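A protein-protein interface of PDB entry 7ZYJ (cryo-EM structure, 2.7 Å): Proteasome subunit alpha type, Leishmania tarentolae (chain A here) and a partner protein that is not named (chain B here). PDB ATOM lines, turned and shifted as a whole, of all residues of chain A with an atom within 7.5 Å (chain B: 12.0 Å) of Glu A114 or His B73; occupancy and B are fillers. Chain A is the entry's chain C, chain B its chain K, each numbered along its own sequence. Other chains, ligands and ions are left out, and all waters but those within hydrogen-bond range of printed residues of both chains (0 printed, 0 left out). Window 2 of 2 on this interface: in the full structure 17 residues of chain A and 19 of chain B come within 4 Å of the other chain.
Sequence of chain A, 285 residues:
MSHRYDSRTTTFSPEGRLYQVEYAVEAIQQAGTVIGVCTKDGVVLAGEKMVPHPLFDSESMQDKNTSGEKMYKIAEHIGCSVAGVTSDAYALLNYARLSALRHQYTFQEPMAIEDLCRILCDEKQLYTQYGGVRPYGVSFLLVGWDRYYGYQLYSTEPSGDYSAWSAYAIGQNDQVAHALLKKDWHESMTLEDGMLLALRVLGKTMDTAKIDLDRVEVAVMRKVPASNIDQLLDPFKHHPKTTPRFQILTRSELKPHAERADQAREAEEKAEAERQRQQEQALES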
ATOM      1  N   MET A 111      30.497 -25.164  18.860  1.00  0.00           N
ATOM      2  CA  MET A 111      29.165 -25.220  19.442  1.00  0.00           C
ATOM      3  C   MET A 111      28.306 -26.247  18.719  1.00  0.00           C
ATOM      4  O   MET A 111      28.361 -26.373  17.492  1.00  0.00           O
ATOM      5  CB  MET A 111      28.500 -23.846  19.379  1.00  0.00           C
ATOM      6  CG  MET A 111      27.517 -23.575  20.502  1.00  0.00           C
ATOM      7  SD  MET A 111      26.682 -21.990  20.314  1.00  0.00           S
ATOM      8  CE  MET A 111      25.792 -21.886  21.863  1.00  0.00           C
ATOM      9  N   ALA A 112      27.513 -26.988  19.486  1.00  0.00           N
ATOM     10  CA  ALA A 112      26.571 -27.923  18.891  1.00  0.00           C
ATOM     11  C   ALA A 112      25.525 -27.167  18.085  1.00  0.00           C
ATOM     12  O   ALA A 112      25.113 -26.064  18.453  1.00  0.00           O
ATOM     13  CB  ALA A 112      25.900 -28.769  19.972  1.00  0.00           C
ATOM     14  N   ILE A 113      25.100 -27.767  16.972  1.00  0.00           N
ATOM     15  CA  ILE A 113      24.130 -27.114  16.096  1.00  0.00           C
ATOM     16  C   ILE A 113      22.817 -26.887  16.832  1.00  0.00           C
ATOM     17  O   ILE A 113      22.203 -25.817  16.725  1.00  0.00           O
ATOM     18  CB  ILE A 113      23.926 -27.942  14.815  1.00  0.00           C
ATOM     19  CG1 ILE A 113      25.278 -28.331  14.212  1.00  0.00           C
ATOM     20  CG2 ILE A 113      23.094 -27.170  13.807  1.00  0.00           C
ATOM     21  CD1 ILE A 113      26.178 -27.153  13.918  1.00  0.00           C
ATOM     22  N   GLU A 114      22.367 -27.886  17.594  1.00  0.00           N
ATOM     23  CA  GLU A 114      21.129 -27.741  18.350  1.00  0.00           C
ATOM     24  C   GLU A 114      21.252 -26.654  19.411  1.00  0.00           C
ATOM     25  O   GLU A 114      20.294 -25.915  19.657  1.00  0.00           O
ATOM     26  CB  GLU A 114      20.745 -29.074  18.989  1.00  0.00           C
ATOM     27  CG  GLU A 114      19.317 -29.120  19.505  1.00  0.00           C
ATOM     28  CD  GLU A 114      19.059 -30.315  20.398  1.00  0.00           C
ATOM     29  OE1 GLU A 114      19.794 -30.486  21.393  1.00  0.00           O
ATOM     30  OE2 GLU A 114      18.121 -31.087  20.104  1.00  0.00           O
ATOM     31  N   ASP A 115      22.419 -26.542  20.050  1.00  0.00           N
ATOM     32  CA  ASP A 115      22.607 -25.501  21.056  1.00  0.00           C
ATOM     33  C   ASP A 115      22.523 -24.109  20.441  1.00  0.00           C
ATOM     34  O   ASP A 115      21.887 -23.212  21.006  1.00  0.00           O
ATOM     35  CB  ASP A 115      23.945 -25.689  21.769  1.00  0.00           C
ATOM     36  CG  ASP A 115      23.968 -26.923  22.648  1.00  0.00           C
ATOM     37  OD1 ASP A 115      22.897 -27.314  23.154  1.00  0.00           O
ATOM     38  OD2 ASP A 115      25.061 -27.497  22.838  1.00  0.00           O
ATOM     39  N   LEU A 116      23.160 -23.907  19.285  1.00  0.00           N
ATOM     40  CA  LEU A 116      23.080 -22.612  18.619  1.00  0.00           C
ATOM     41  C   LEU A 116      21.658 -22.322  18.159  1.00  0.00           C
ATOM     42  O   LEU A 116      21.184 -21.183  18.249  1.00  0.00           O
ATOM     43  CB  LEU A 116      24.039 -22.554  17.433  1.00  0.00           C
ATOM     44  CG  LEU A 116      23.935 -21.217  16.695  1.00  0.00           C
ATOM     45  CD1 LEU A 116      24.678 -20.121  17.449  1.00  0.00           C
ATOM     46  CD2 LEU A 116      24.415 -21.323  15.269  1.00  0.00           C
ATOM     47  N   CYS A 117      20.963 -23.339  17.648  1.00  0.00           N
ATOM     48  CA  CYS A 117      19.575 -23.142  17.247  1.00  0.00           C
ATOM     49  C   CYS A 117      18.717 -22.742  18.439  1.00  0.00           C
ATOM     50  O   CYS A 117      17.857 -21.863  18.329  1.00  0.00           O
ATOM     51  CB  CYS A 117      19.034 -24.413  16.592  1.00  0.00           C
ATOM     52  SG  CYS A 117      17.334 -24.282  16.014  1.00  0.00           S
ATOM     53  N   ARG A 118      18.945 -23.373  19.591  1.00  0.00           N
ATOM     54  CA  ARG A 118      18.178 -23.048  20.788  1.00  0.00           C
ATOM     55  C   ARG A 118      18.483 -21.642  21.288  1.00  0.00           C
ATOM     56  O   ARG A 118      17.572 -20.918  21.703  1.00  0.00           O
ATOM     57  CB  ARG A 118      18.464 -24.076  21.881  1.00  0.00           C
ATOM     58  CG  ARG A 118      17.773 -23.792  23.200  1.00  0.00           C
ATOM     59  CD  ARG A 118      18.093 -24.864  24.226  1.00  0.00           C
ATOM     60  NE  ARG A 118      19.530 -25.007  24.422  1.00  0.00           N
ATOM     61  CZ  ARG A 118      20.209 -24.454  25.417  1.00  0.00           C
ATOM     62  NH1 ARG A 118      19.610 -23.712  26.334  1.00  0.00           N
ATOM     63  NH2 ARG A 118      21.522 -24.647  25.493  1.00  0.00           N
ATOM     64  N   ILE A 119      19.756 -21.234  21.257  1.00  0.00           N
ATOM     65  CA  ILE A 119      20.123 -19.965  21.880  1.00  0.00           C
ATOM     66  C   ILE A 119      19.548 -18.782  21.105  1.00  0.00           C
ATOM     67  O   ILE A 119      19.161 -17.774  21.708  1.00  0.00           O
ATOM     68  CB  ILE A 119      21.652 -19.857  22.051  1.00  0.00           C
ATOM     69  CG1 ILE A 119      22.006 -18.658  22.930  1.00  0.00           C
ATOM     70  CG2 ILE A 119      22.356 -19.729  20.717  1.00  0.00           C
ATOM     71  CD1 ILE A 119      23.436 -18.660  23.409  1.00  0.00           C
ATOM     72  N   LEU A 120      19.474 -18.871  19.776  1.00  0.00           N
ATOM     73  CA  LEU A 120      18.878 -17.799  18.990  1.00  0.00           C
ATOM     74  C   LEU A 120      17.360 -17.894  18.916  1.00  0.00           C
ATOM     75  O   LEU A 120      16.716 -16.925  18.504  1.00  0.00           O
ATOM     76  CB  LEU A 120      19.470 -17.774  17.571  1.00  0.00           C
ATOM     77  CG  LEU A 120      19.309 -18.953  16.607  1.00  0.00           C
ATOM     78  CD1 LEU A 120      17.983 -18.914  15.857  1.00  0.00           C
ATOM     79  CD2 LEU A 120      20.468 -18.978  15.625  1.00  0.00           C
ATOM     80  N   CYS A 121      16.779 -19.030  19.298  1.00  0.00           N
ATOM     81  CA  CYS A 121      15.328 -19.119  19.402  1.00  0.00           C
ATOM     82  C   CYS A 121      14.810 -18.456  20.669  1.00  0.00           C
ATOM     83  O   CYS A 121      13.704 -17.903  20.665  1.00  0.00           O
ATOM     84  CB  CYS A 121      14.883 -20.579  19.347  1.00  0.00           C
ATOM     85  SG  CYS A 121      14.831 -21.256  17.680  1.00  0.00           S
ATOM     86  N   LEU A 142      18.986 -23.724   9.529  1.00  0.00           N
ATOM     87  CA  LEU A 142      20.330 -23.936  10.049  1.00  0.00           C
ATOM     88  C   LEU A 142      20.873 -25.267   9.551  1.00  0.00           C
ATOM     89  O   LEU A 142      20.166 -26.279   9.573  1.00  0.00           O
ATOM     90  CB  LEU A 142      20.346 -23.919  11.578  1.00  0.00           C
ATOM     91  CG  LEU A 142      20.286 -22.578  12.310  1.00  0.00           C
ATOM     92  CD1 LEU A 142      18.864 -22.061  12.360  1.00  0.00           C
ATOM     93  CD2 LEU A 142      20.858 -22.715  13.709  1.00  0.00           C
ATOM     94  N   ASP A 146      28.289 -31.570  13.875  1.00  0.00           N
ATOM     95  CA  ASP A 146      28.940 -31.710  15.169  1.00  0.00           C
ATOM     96  C   ASP A 146      29.100 -33.193  15.466  1.00  0.00           C
ATOM     97  O   ASP A 146      28.377 -34.034  14.927  1.00  0.00           O
ATOM     98  CB  ASP A 146      28.163 -31.001  16.286  1.00  0.00           C
ATOM     99  CG  ASP A 146      26.731 -31.477  16.398  1.00  0.00           C
ATOM    100  OD1 ASP A 146      26.266 -32.205  15.497  1.00  0.00           O
ATOM    101  OD2 ASP A 146      26.065 -31.120  17.391  1.00  0.00           O
ATOM    102  N   TYR A 149      25.809 -35.524  16.649  1.00  0.00           N
ATOM    103  CA  TYR A 149      24.765 -35.975  15.743  1.00  0.00           C
ATOM    104  C   TYR A 149      25.136 -35.866  14.272  1.00  0.00           C
ATOM    105  O   TYR A 149      24.285 -36.134  13.418  1.00  0.00           O
ATOM    106  CB  TYR A 149      23.464 -35.196  15.990  1.00  0.00           C
ATOM    107  CG  TYR A 149      23.031 -35.177  17.435  1.00  0.00           C
ATOM    108  CD1 TYR A 149      22.699 -36.351  18.095  1.00  0.00           C
ATOM    109  CD2 TYR A 149      22.949 -33.985  18.140  1.00  0.00           C
ATOM    110  CE1 TYR A 149      22.300 -36.340  19.416  1.00  0.00           C
ATOM    111  CE2 TYR A 149      22.552 -33.964  19.462  1.00  0.00           C
ATOM    112  CZ  TYR A 149      22.228 -35.144  20.094  1.00  0.00           C
ATOM    113  OH  TYR A 149      21.831 -35.131  21.411  1.00  0.00           O
ATOM    114  N   GLN A 152      23.171 -31.983  10.505  1.00  0.00           N
ATOM    115  CA  GLN A 152      21.871 -31.651  11.069  1.00  0.00           C
ATOM    116  C   GLN A 152      21.219 -30.543  10.253  1.00  0.00           C
ATOM    117  O   GLN A 152      21.877 -29.808   9.514  1.00  0.00           O
ATOM    118  CB  GLN A 152      21.988 -31.224  12.538  1.00  0.00           C
ATOM    119  CG  GLN A 152      22.660 -32.246  13.436  1.00  0.00           C
ATOM    120  CD  GLN A 152      22.648 -31.835  14.890  1.00  0.00           C
ATOM    121  OE1 GLN A 152      21.590 -31.705  15.499  1.00  0.00           O
ATOM    122  NE2 GLN A 152      23.829 -31.623  15.452  1.00  0.00           N
ATOM    123  N   TYR A 154      17.927 -27.647  10.886  1.00  0.00           N
ATOM    124  CA  TYR A 154      16.921 -27.088  11.772  1.00  0.00           C
ATOM    125  C   TYR A 154      16.171 -25.956  11.084  1.00  0.00           C
ATOM    126  O   TYR A 154      16.709 -25.248  10.228  1.00  0.00           O
ATOM    127  CB  TYR A 154      17.548 -26.578  13.076  1.00  0.00           C
ATOM    128  CG  TYR A 154      18.123 -27.673  13.940  1.00  0.00           C
ATOM    129  CD1 TYR A 154      19.430 -28.103  13.769  1.00  0.00           C
ATOM    130  CD2 TYR A 154      17.357 -28.281  14.924  1.00  0.00           C
ATOM    131  CE1 TYR A 154      19.959 -29.104  14.554  1.00  0.00           C
ATOM    132  CE2 TYR A 154      17.877 -29.284  15.713  1.00  0.00           C
ATOM    133  CZ  TYR A 154      19.179 -29.692  15.525  1.00  0.00           C
ATOM    134  OH  TYR A 154      19.703 -30.692  16.309  1.00  0.00           O
ATOM    135  N   TYR A 162      11.480 -24.194  17.280  1.00  0.00           N
ATOM    136  CA  TYR A 162      12.392 -24.751  16.297  1.00  0.00           C
ATOM    137  C   TYR A 162      12.146 -26.247  16.177  1.00  0.00           C
ATOM    138  O   TYR A 162      11.609 -26.886  17.084  1.00  0.00           O
ATOM    139  CB  TYR A 162      13.860 -24.477  16.653  1.00  0.00           C
ATOM    140  CG  TYR A 162      14.368 -25.232  17.860  1.00  0.00           C
ATOM    141  CD1 TYR A 162      14.177 -24.739  19.143  1.00  0.00           C
ATOM    142  CD2 TYR A 162      15.056 -26.430  17.715  1.00  0.00           C
ATOM    143  CE1 TYR A 162      14.643 -25.421  20.247  1.00  0.00           C
ATOM    144  CE2 TYR A 162      15.528 -27.119  18.815  1.00  0.00           C
ATOM    145  CZ  TYR A 162      15.318 -26.610  20.078  1.00  0.00           C
ATOM    146  OH  TYR A 162      15.786 -27.292  21.177  1.00  0.00           O
ATOM    147  N   ALA A 164      13.783 -30.033  14.081  1.00  0.00           N
ATOM    148  CA  ALA A 164      14.816 -30.703  13.308  1.00  0.00           C
ATOM    149  C   ALA A 164      14.176 -31.478  12.167  1.00  0.00           C
ATOM    150  O   ALA A 164      13.150 -32.140  12.348  1.00  0.00           O
ATOM    151  CB  ALA A 164      15.633 -31.645  14.191  1.00  0.00           C
ATOM    152  N   ASP B  40      32.060 -35.845  36.323  1.00  0.00           N
ATOM    153  CA  ASP B  40      31.198 -36.559  35.395  1.00  0.00           C
ATOM    154  C   ASP B  40      31.409 -38.054  35.602  1.00  0.00           C
ATOM    155  O   ASP B  40      32.134 -38.453  36.518  1.00  0.00           O
ATOM    156  CB  ASP B  40      31.504 -36.129  33.955  1.00  0.00           C
ATOM    157  CG  ASP B  40      30.492 -36.649  32.954  1.00  0.00           C
ATOM    158  OD1 ASP B  40      29.356 -36.130  32.931  1.00  0.00           O
ATOM    159  OD2 ASP B  40      30.833 -37.574  32.188  1.00  0.00           O
ATOM    160  N   ASN B  64      27.526 -26.792  37.113  1.00  0.00           N
ATOM    161  CA  ASN B  64      27.456 -26.256  35.758  1.00  0.00           C
ATOM    162  C   ASN B  64      27.532 -27.366  34.718  1.00  0.00           C
ATOM    163  O   ASN B  64      26.828 -27.318  33.702  1.00  0.00           O
ATOM    164  CB  ASN B  64      28.563 -25.228  35.541  1.00  0.00           C
ATOM    165  CG  ASN B  64      28.215 -23.875  36.120  1.00  0.00           C
ATOM    166  OD1 ASN B  64      27.836 -22.956  35.396  1.00  0.00           O
ATOM    167  ND2 ASN B  64      28.332 -23.747  37.435  1.00  0.00           N
ATOM    168  N   LEU B  65      28.372 -28.377  34.952  1.00  0.00           N
ATOM    169  CA  LEU B  65      28.424 -29.511  34.034  1.00  0.00           C
ATOM    170  C   LEU B  65      27.092 -30.249  33.993  1.00  0.00           C
ATOM    171  O   LEU B  65      26.615 -30.632  32.918  1.00  0.00           O
ATOM    172  CB  LEU B  65      29.547 -30.465  34.432  1.00  0.00           C
ATOM    173  CG  LEU B  65      30.980 -29.964  34.274  1.00  0.00           C
ATOM    174  CD1 LEU B  65      31.944 -30.966  34.878  1.00  0.00           C
ATOM    175  CD2 LEU B  65      31.303 -29.710  32.812  1.00  0.00           C
ATOM    176  N   ALA B  66      26.478 -30.462  35.160  1.00  0.00           N
ATOM    177  CA  ALA B  66      25.180 -31.128  35.200  1.00  0.00           C
ATOM    178  C   ALA B  66      24.116 -30.309  34.482  1.00  0.00           C
ATOM    179  O   ALA B  66      23.281 -30.861  33.756  1.00  0.00           O
ATOM    180  CB  ALA B  66      24.771 -31.392  36.649  1.00  0.00           C
ATOM    181  N   LEU B  67      24.127 -28.988  34.675  1.00  0.00           N
ATOM    182  CA  LEU B  67      23.164 -28.130  33.993  1.00  0.00           C
ATOM    183  C   LEU B  67      23.357 -28.176  32.484  1.00  0.00           C
ATOM    184  O   LEU B  67      22.378 -28.202  31.728  1.00  0.00           O
ATOM    185  CB  LEU B  67      23.283 -26.697  34.508  1.00  0.00           C
ATOM    186  CG  LEU B  67      22.292 -25.677  33.947  1.00  0.00           C
ATOM    187  CD1 LEU B  67      20.881 -26.240  33.949  1.00  0.00           C
ATOM    188  CD2 LEU B  67      22.354 -24.390  34.746  1.00  0.00           C
ATOM    189  N   ASN B  68      24.611 -28.174  32.027  1.00  0.00           N
ATOM    190  CA  ASN B  68      24.870 -28.294  30.596  1.00  0.00           C
ATOM    191  C   ASN B  68      24.371 -29.627  30.058  1.00  0.00           C
ATOM    192  O   ASN B  68      23.775 -29.684  28.979  1.00  0.00           O
ATOM    193  CB  ASN B  68      26.361 -28.123  30.312  1.00  0.00           C
ATOM    194  CG  ASN B  68      26.860 -26.733  30.645  1.00  0.00           C
ATOM    195  OD1 ASN B  68      26.101 -25.884  31.109  1.00  0.00           O
ATOM    196  ND2 ASN B  68      28.143 -26.493  30.408  1.00  0.00           N
ATOM    197  N   ARG B  69      24.597 -30.713  30.802  1.00  0.00           N
ATOM    198  CA  ARG B  69      24.090 -32.011  30.371  1.00  0.00           C
ATOM    199  C   ARG B  69      22.567 -32.011  30.293  1.00  0.00           C
ATOM    200  O   ARG B  69      21.985 -32.618  29.386  1.00  0.00           O
ATOM    201  CB  ARG B  69      24.579 -33.110  31.313  1.00  0.00           C
ATOM    202  CG  ARG B  69      25.958 -33.645  30.973  1.00  0.00           C
ATOM    203  CD  ARG B  69      26.174 -35.032  31.561  1.00  0.00           C
ATOM    204  NE  ARG B  69      25.705 -35.137  32.938  1.00  0.00           N
ATOM    205  CZ  ARG B  69      26.296 -34.568  33.983  1.00  0.00           C
ATOM    206  NH1 ARG B  69      27.401 -33.853  33.849  1.00  0.00           N
ATOM    207  NH2 ARG B  69      25.767 -34.728  35.192  1.00  0.00           N
ATOM    208  N   MET B  70      21.907 -31.345  31.241  1.00  0.00           N
ATOM    209  CA  MET B  70      20.452 -31.242  31.201  1.00  0.00           C
ATOM    210  C   MET B  70      19.990 -30.473  29.968  1.00  0.00           C
ATOM    211  O   MET B  70      19.096 -30.917  29.239  1.00  0.00           O
ATOM    212  CB  MET B  70      19.934 -30.571  32.476  1.00  0.00           C
ATOM    213  CG  MET B  70      20.172 -31.366  33.744  1.00  0.00           C
ATOM    214  SD  MET B  70      19.297 -32.939  33.767  1.00  0.00           S
ATOM    215  CE  MET B  70      19.986 -33.675  35.246  1.00  0.00           C
ATOM    216  N   ARG B  71      20.596 -29.312  29.717  1.00  0.00           N
ATOM    217  CA  ARG B  71      20.190 -28.478  28.591  1.00  0.00           C
ATOM    218  C   ARG B  71      20.676 -29.002  27.249  1.00  0.00           C
ATOM    219  O   ARG B  71      20.257 -28.473  26.214  1.00  0.00           O
ATOM    220  CB  ARG B  71      20.678 -27.044  28.793  1.00  0.00           C
ATOM    221  CG  ARG B  71      19.808 -26.225  29.729  1.00  0.00           C
ATOM    222  CD  ARG B  71      20.593 -25.105  30.384  1.00  0.00           C
ATOM    223  NE  ARG B  71      19.766 -24.332  31.303  1.00  0.00           N
ATOM    224  CZ  ARG B  71      20.148 -23.203  31.886  1.00  0.00           C
ATOM    225  NH1 ARG B  71      21.346 -22.685  31.671  1.00  0.00           N
ATOM    226  NH2 ARG B  71      19.306 -22.579  32.705  1.00  0.00           N
ATOM    227  N   GLN B  72      21.542 -30.017  27.230  1.00  0.00           N
ATOM    228  CA  GLN B  72      22.001 -30.623  25.986  1.00  0.00           C
ATOM    229  C   GLN B  72      21.505 -32.056  25.834  1.00  0.00           C
ATOM    230  O   GLN B  72      22.066 -32.821  25.045  1.00  0.00           O
ATOM    231  CB  GLN B  72      23.526 -30.571  25.890  1.00  0.00           C
ATOM    232  CG  GLN B  72      24.099 -29.164  25.948  1.00  0.00           C
ATOM    233  CD  GLN B  72      25.613 -29.150  25.891  1.00  0.00           C
ATOM    234  OE1 GLN B  72      26.251 -30.195  25.773  1.00  0.00           O
ATOM    235  NE2 GLN B  72      26.195 -27.961  25.976  1.00  0.00           N
ATOM    236  N   HIS B  73      20.462 -32.430  26.578  1.00  0.00           N
ATOM    237  CA  HIS B  73      19.816 -33.738  26.466  1.00  0.00           C
ATOM    238  C   HIS B  73      20.809 -34.875  26.719  1.00  0.00           C
ATOM    239  O   HIS B  73      20.967 -35.796  25.914  1.00  0.00           O
ATOM    240  CB  HIS B  73      19.131 -33.892  25.104  1.00  0.00           C
ATOM    241  CG  HIS B  73      18.202 -32.769  24.767  1.00  0.00           C
ATOM    242  ND1 HIS B  73      18.279 -32.067  23.584  1.00  0.00           N
ATOM    243  CD2 HIS B  73      17.177 -32.221  25.462  1.00  0.00           C
ATOM    244  CE1 HIS B  73      17.340 -31.138  23.563  1.00  0.00           C
ATOM    245  NE2 HIS B  73      16.658 -31.210  24.691  1.00  0.00           N
ATOM    246  N   GLY B  74      21.481 -34.793  27.864  1.00  0.00           N
ATOM    247  CA  GLY B  74      22.362 -35.863  28.294  1.00  0.00           C
ATOM    248  C   GLY B  74      23.627 -36.020  27.485  1.00  0.00           C
ATOM    249  O   GLY B  74      24.232 -37.095  27.502  1.00  0.00           O
ATOM    250  N   ARG B  75      24.051 -34.979  26.774  1.00  0.00           N
ATOM    251  CA  ARG B  75      25.285 -35.032  25.997  1.00  0.00           C
ATOM    252  C   ARG B  75      26.460 -34.729  26.919  1.00  0.00           C
ATOM    253  O   ARG B  75      26.573 -33.618  27.446  1.00  0.00           O
ATOM    254  CB  ARG B  75      25.225 -34.051  24.830  1.00  0.00           C
ATOM    255  CG  ARG B  75      24.315 -34.497  23.699  1.00  0.00           C
ATOM    256  CD  ARG B  75      24.552 -33.689  22.436  1.00  0.00           C
ATOM    257  NE  ARG B  75      23.734 -32.484  22.384  1.00  0.00           N
ATOM    258  CZ  ARG B  75      24.195 -31.256  22.580  1.00  0.00           C
ATOM    259  NH1 ARG B  75      25.470 -31.033  22.856  1.00  0.00           N
ATOM    260  NH2 ARG B  75      23.356 -30.227  22.499  1.00  0.00           N
ATOM    261  N   HIS B  76      27.331 -35.714  27.118  1.00  0.00           N
ATOM    262  CA  HIS B  76      28.462 -35.553  28.019  1.00  0.00           C
ATOM    263  C   HIS B  76      29.575 -34.759  27.348  1.00  0.00           C
ATOM    264  O   HIS B  76      29.864 -34.942  26.163  1.00  0.00           O
ATOM    265  CB  HIS B  76      28.983 -36.917  28.470  1.00  0.00           C
ATOM    266  CG  HIS B  76      28.097 -37.597  29.467  1.00  0.00           C
ATOM    267  ND1 HIS B  76      28.456 -37.770  30.786  1.00  0.00           N
ATOM    268  CD2 HIS B  76      26.865 -38.143  29.338  1.00  0.00           C
ATOM    269  CE1 HIS B  76      27.484 -38.394  31.427  1.00  0.00           C
ATOM    270  NE2 HIS B  76      26.508 -38.633  30.571  1.00  0.00           N
ATOM    271  N   SER B  77      30.196 -33.871  28.118  1.00  0.00           N
ATOM    272  CA  SER B  77      31.233 -32.989  27.605  1.00  0.00           C
ATOM    273  C   SER B  77      32.587 -33.685  27.609  1.00  0.00           C
ATOM    274  O   SER B  77      32.868 -34.543  28.450  1.00  0.00           O
ATOM    275  CB  SER B  77      31.305 -31.708  28.437  1.00  0.00           C
ATOM    276  OG  SER B  77      32.013 -30.692  27.750  1.00  0.00           O
ATOM    277  N   VAL B 114      31.107 -40.257  21.927  1.00  0.00           N
ATOM    278  CA  VAL B 114      29.734 -39.981  22.337  1.00  0.00           C
ATOM    279  C   VAL B 114      28.742 -40.565  21.340  1.00  0.00           C
ATOM    280  O   VAL B 114      27.627 -40.948  21.715  1.00  0.00           O
ATOM    281  CB  VAL B 114      29.522 -38.468  22.530  1.00  0.00           C
ATOM    282  CG1 VAL B 114      30.400 -37.952  23.657  1.00  0.00           C
ATOM    283  CG2 VAL B 114      29.811 -37.714  21.241  1.00  0.00           C
ATOM    284  N   SER B 115      29.117 -40.640  20.066  1.00  0.00           N
ATOM    285  CA  SER B 115      28.259 -41.206  19.038  1.00  0.00           C
ATOM    286  C   SER B 115      29.142 -41.815  17.957  1.00  0.00           C
ATOM    287  O   SER B 115      30.373 -41.742  18.017  1.00  0.00           O
ATOM    288  CB  SER B 115      27.315 -40.148  18.459  1.00  0.00           C
ATOM    289  OG  SER B 115      28.029 -39.175  17.718  1.00  0.00           O
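Hydrophobic or aromatic side chains of chain A that line the printed part of chain B: Ala A112 and Tyr A149.
Among the printed residues, 7 pairs touch across the chains.
Among the printed residues, Asp or Glu carboxylates within 4 Å of a Lys or Arg side-chain nitrogen of the other chain: Glu A114 with Arg B75 (3.7 Å) and Asp A115 with Arg B75 (3.0 Å).
The guanidinium group (NH1) of Arg B75 lies within hydrogen-bond range of the side-chain amide oxygen (OE1) of Gln B72 (3.1 Å).
The guanidinium group (NH2) of Arg A118 is in salt-bridge range of the side-chain carboxylate (OD1) of Asp A115, at 3.8 Å.
The guanidinium group (NE) of Arg B75 sits close to the side-chain hydroxyl (OH) of Tyr A149 (3.4 Å).
ND1 of His B73 lies within hydrogen-bond range of OE1 of Glu A114 (3.1 Å).
NH2 of Arg B75 is in salt-bridge range of OE1 of Glu A114 (3.7 Å).
The side-chain carboxylate (OD2) of Asp A115 sits at hydrogen-bond distance from the side-chain amide nitrogen (NE2) of Gln B72, 3.4 Å away.
The guanidinium group of Arg B75 is in salt-bridge range of the side-chain carboxylate of Asp A115, at 3.0 Å.
Of chain B, only His B73 and Arg B75 come within 4 Å of Glu A114.
Printed residues of chain A within 4 Å of His B73: Glu A114 (3.1 Å).
No residue of chain B comes within 4 Å of Ile A113.
No residue of chain B comes within 4 Å of Leu A116.
No residue of chain B comes within 4 Å of Cys A117.
Arg A118 touches just one residue of chain B: Arg B71 (3.97 Å).
Of the printed residues of chain A, Arg B75 touches Ala A112, Glu A114, Asp A115 and Tyr A149.
Printed residues of chain A within 4 Å of Gln B72: Asp A115.
Printed residues of chain B within 4 Å of Tyr A149: Arg B75 (3.2 Å).
Printed residues of chain A within 4 Å of Arg B71: Arg A118 (3.97 Å).
The nearest residue of chain B that does not touch Glu A114 is Gln B72 (4.9 Å).
The nearest residue of chain A that does not touch His B73 is Tyr A149 (4.6 Å).
The nearest printed residue of chain A that does not touch Gln B72 is Tyr A149 (4.3 Å).
Among the printed residues, pairs that only touch across the chains: Ala A112 with Arg B75 (3.7 Å) and Arg A118 with Arg B71 (3.97 Å).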
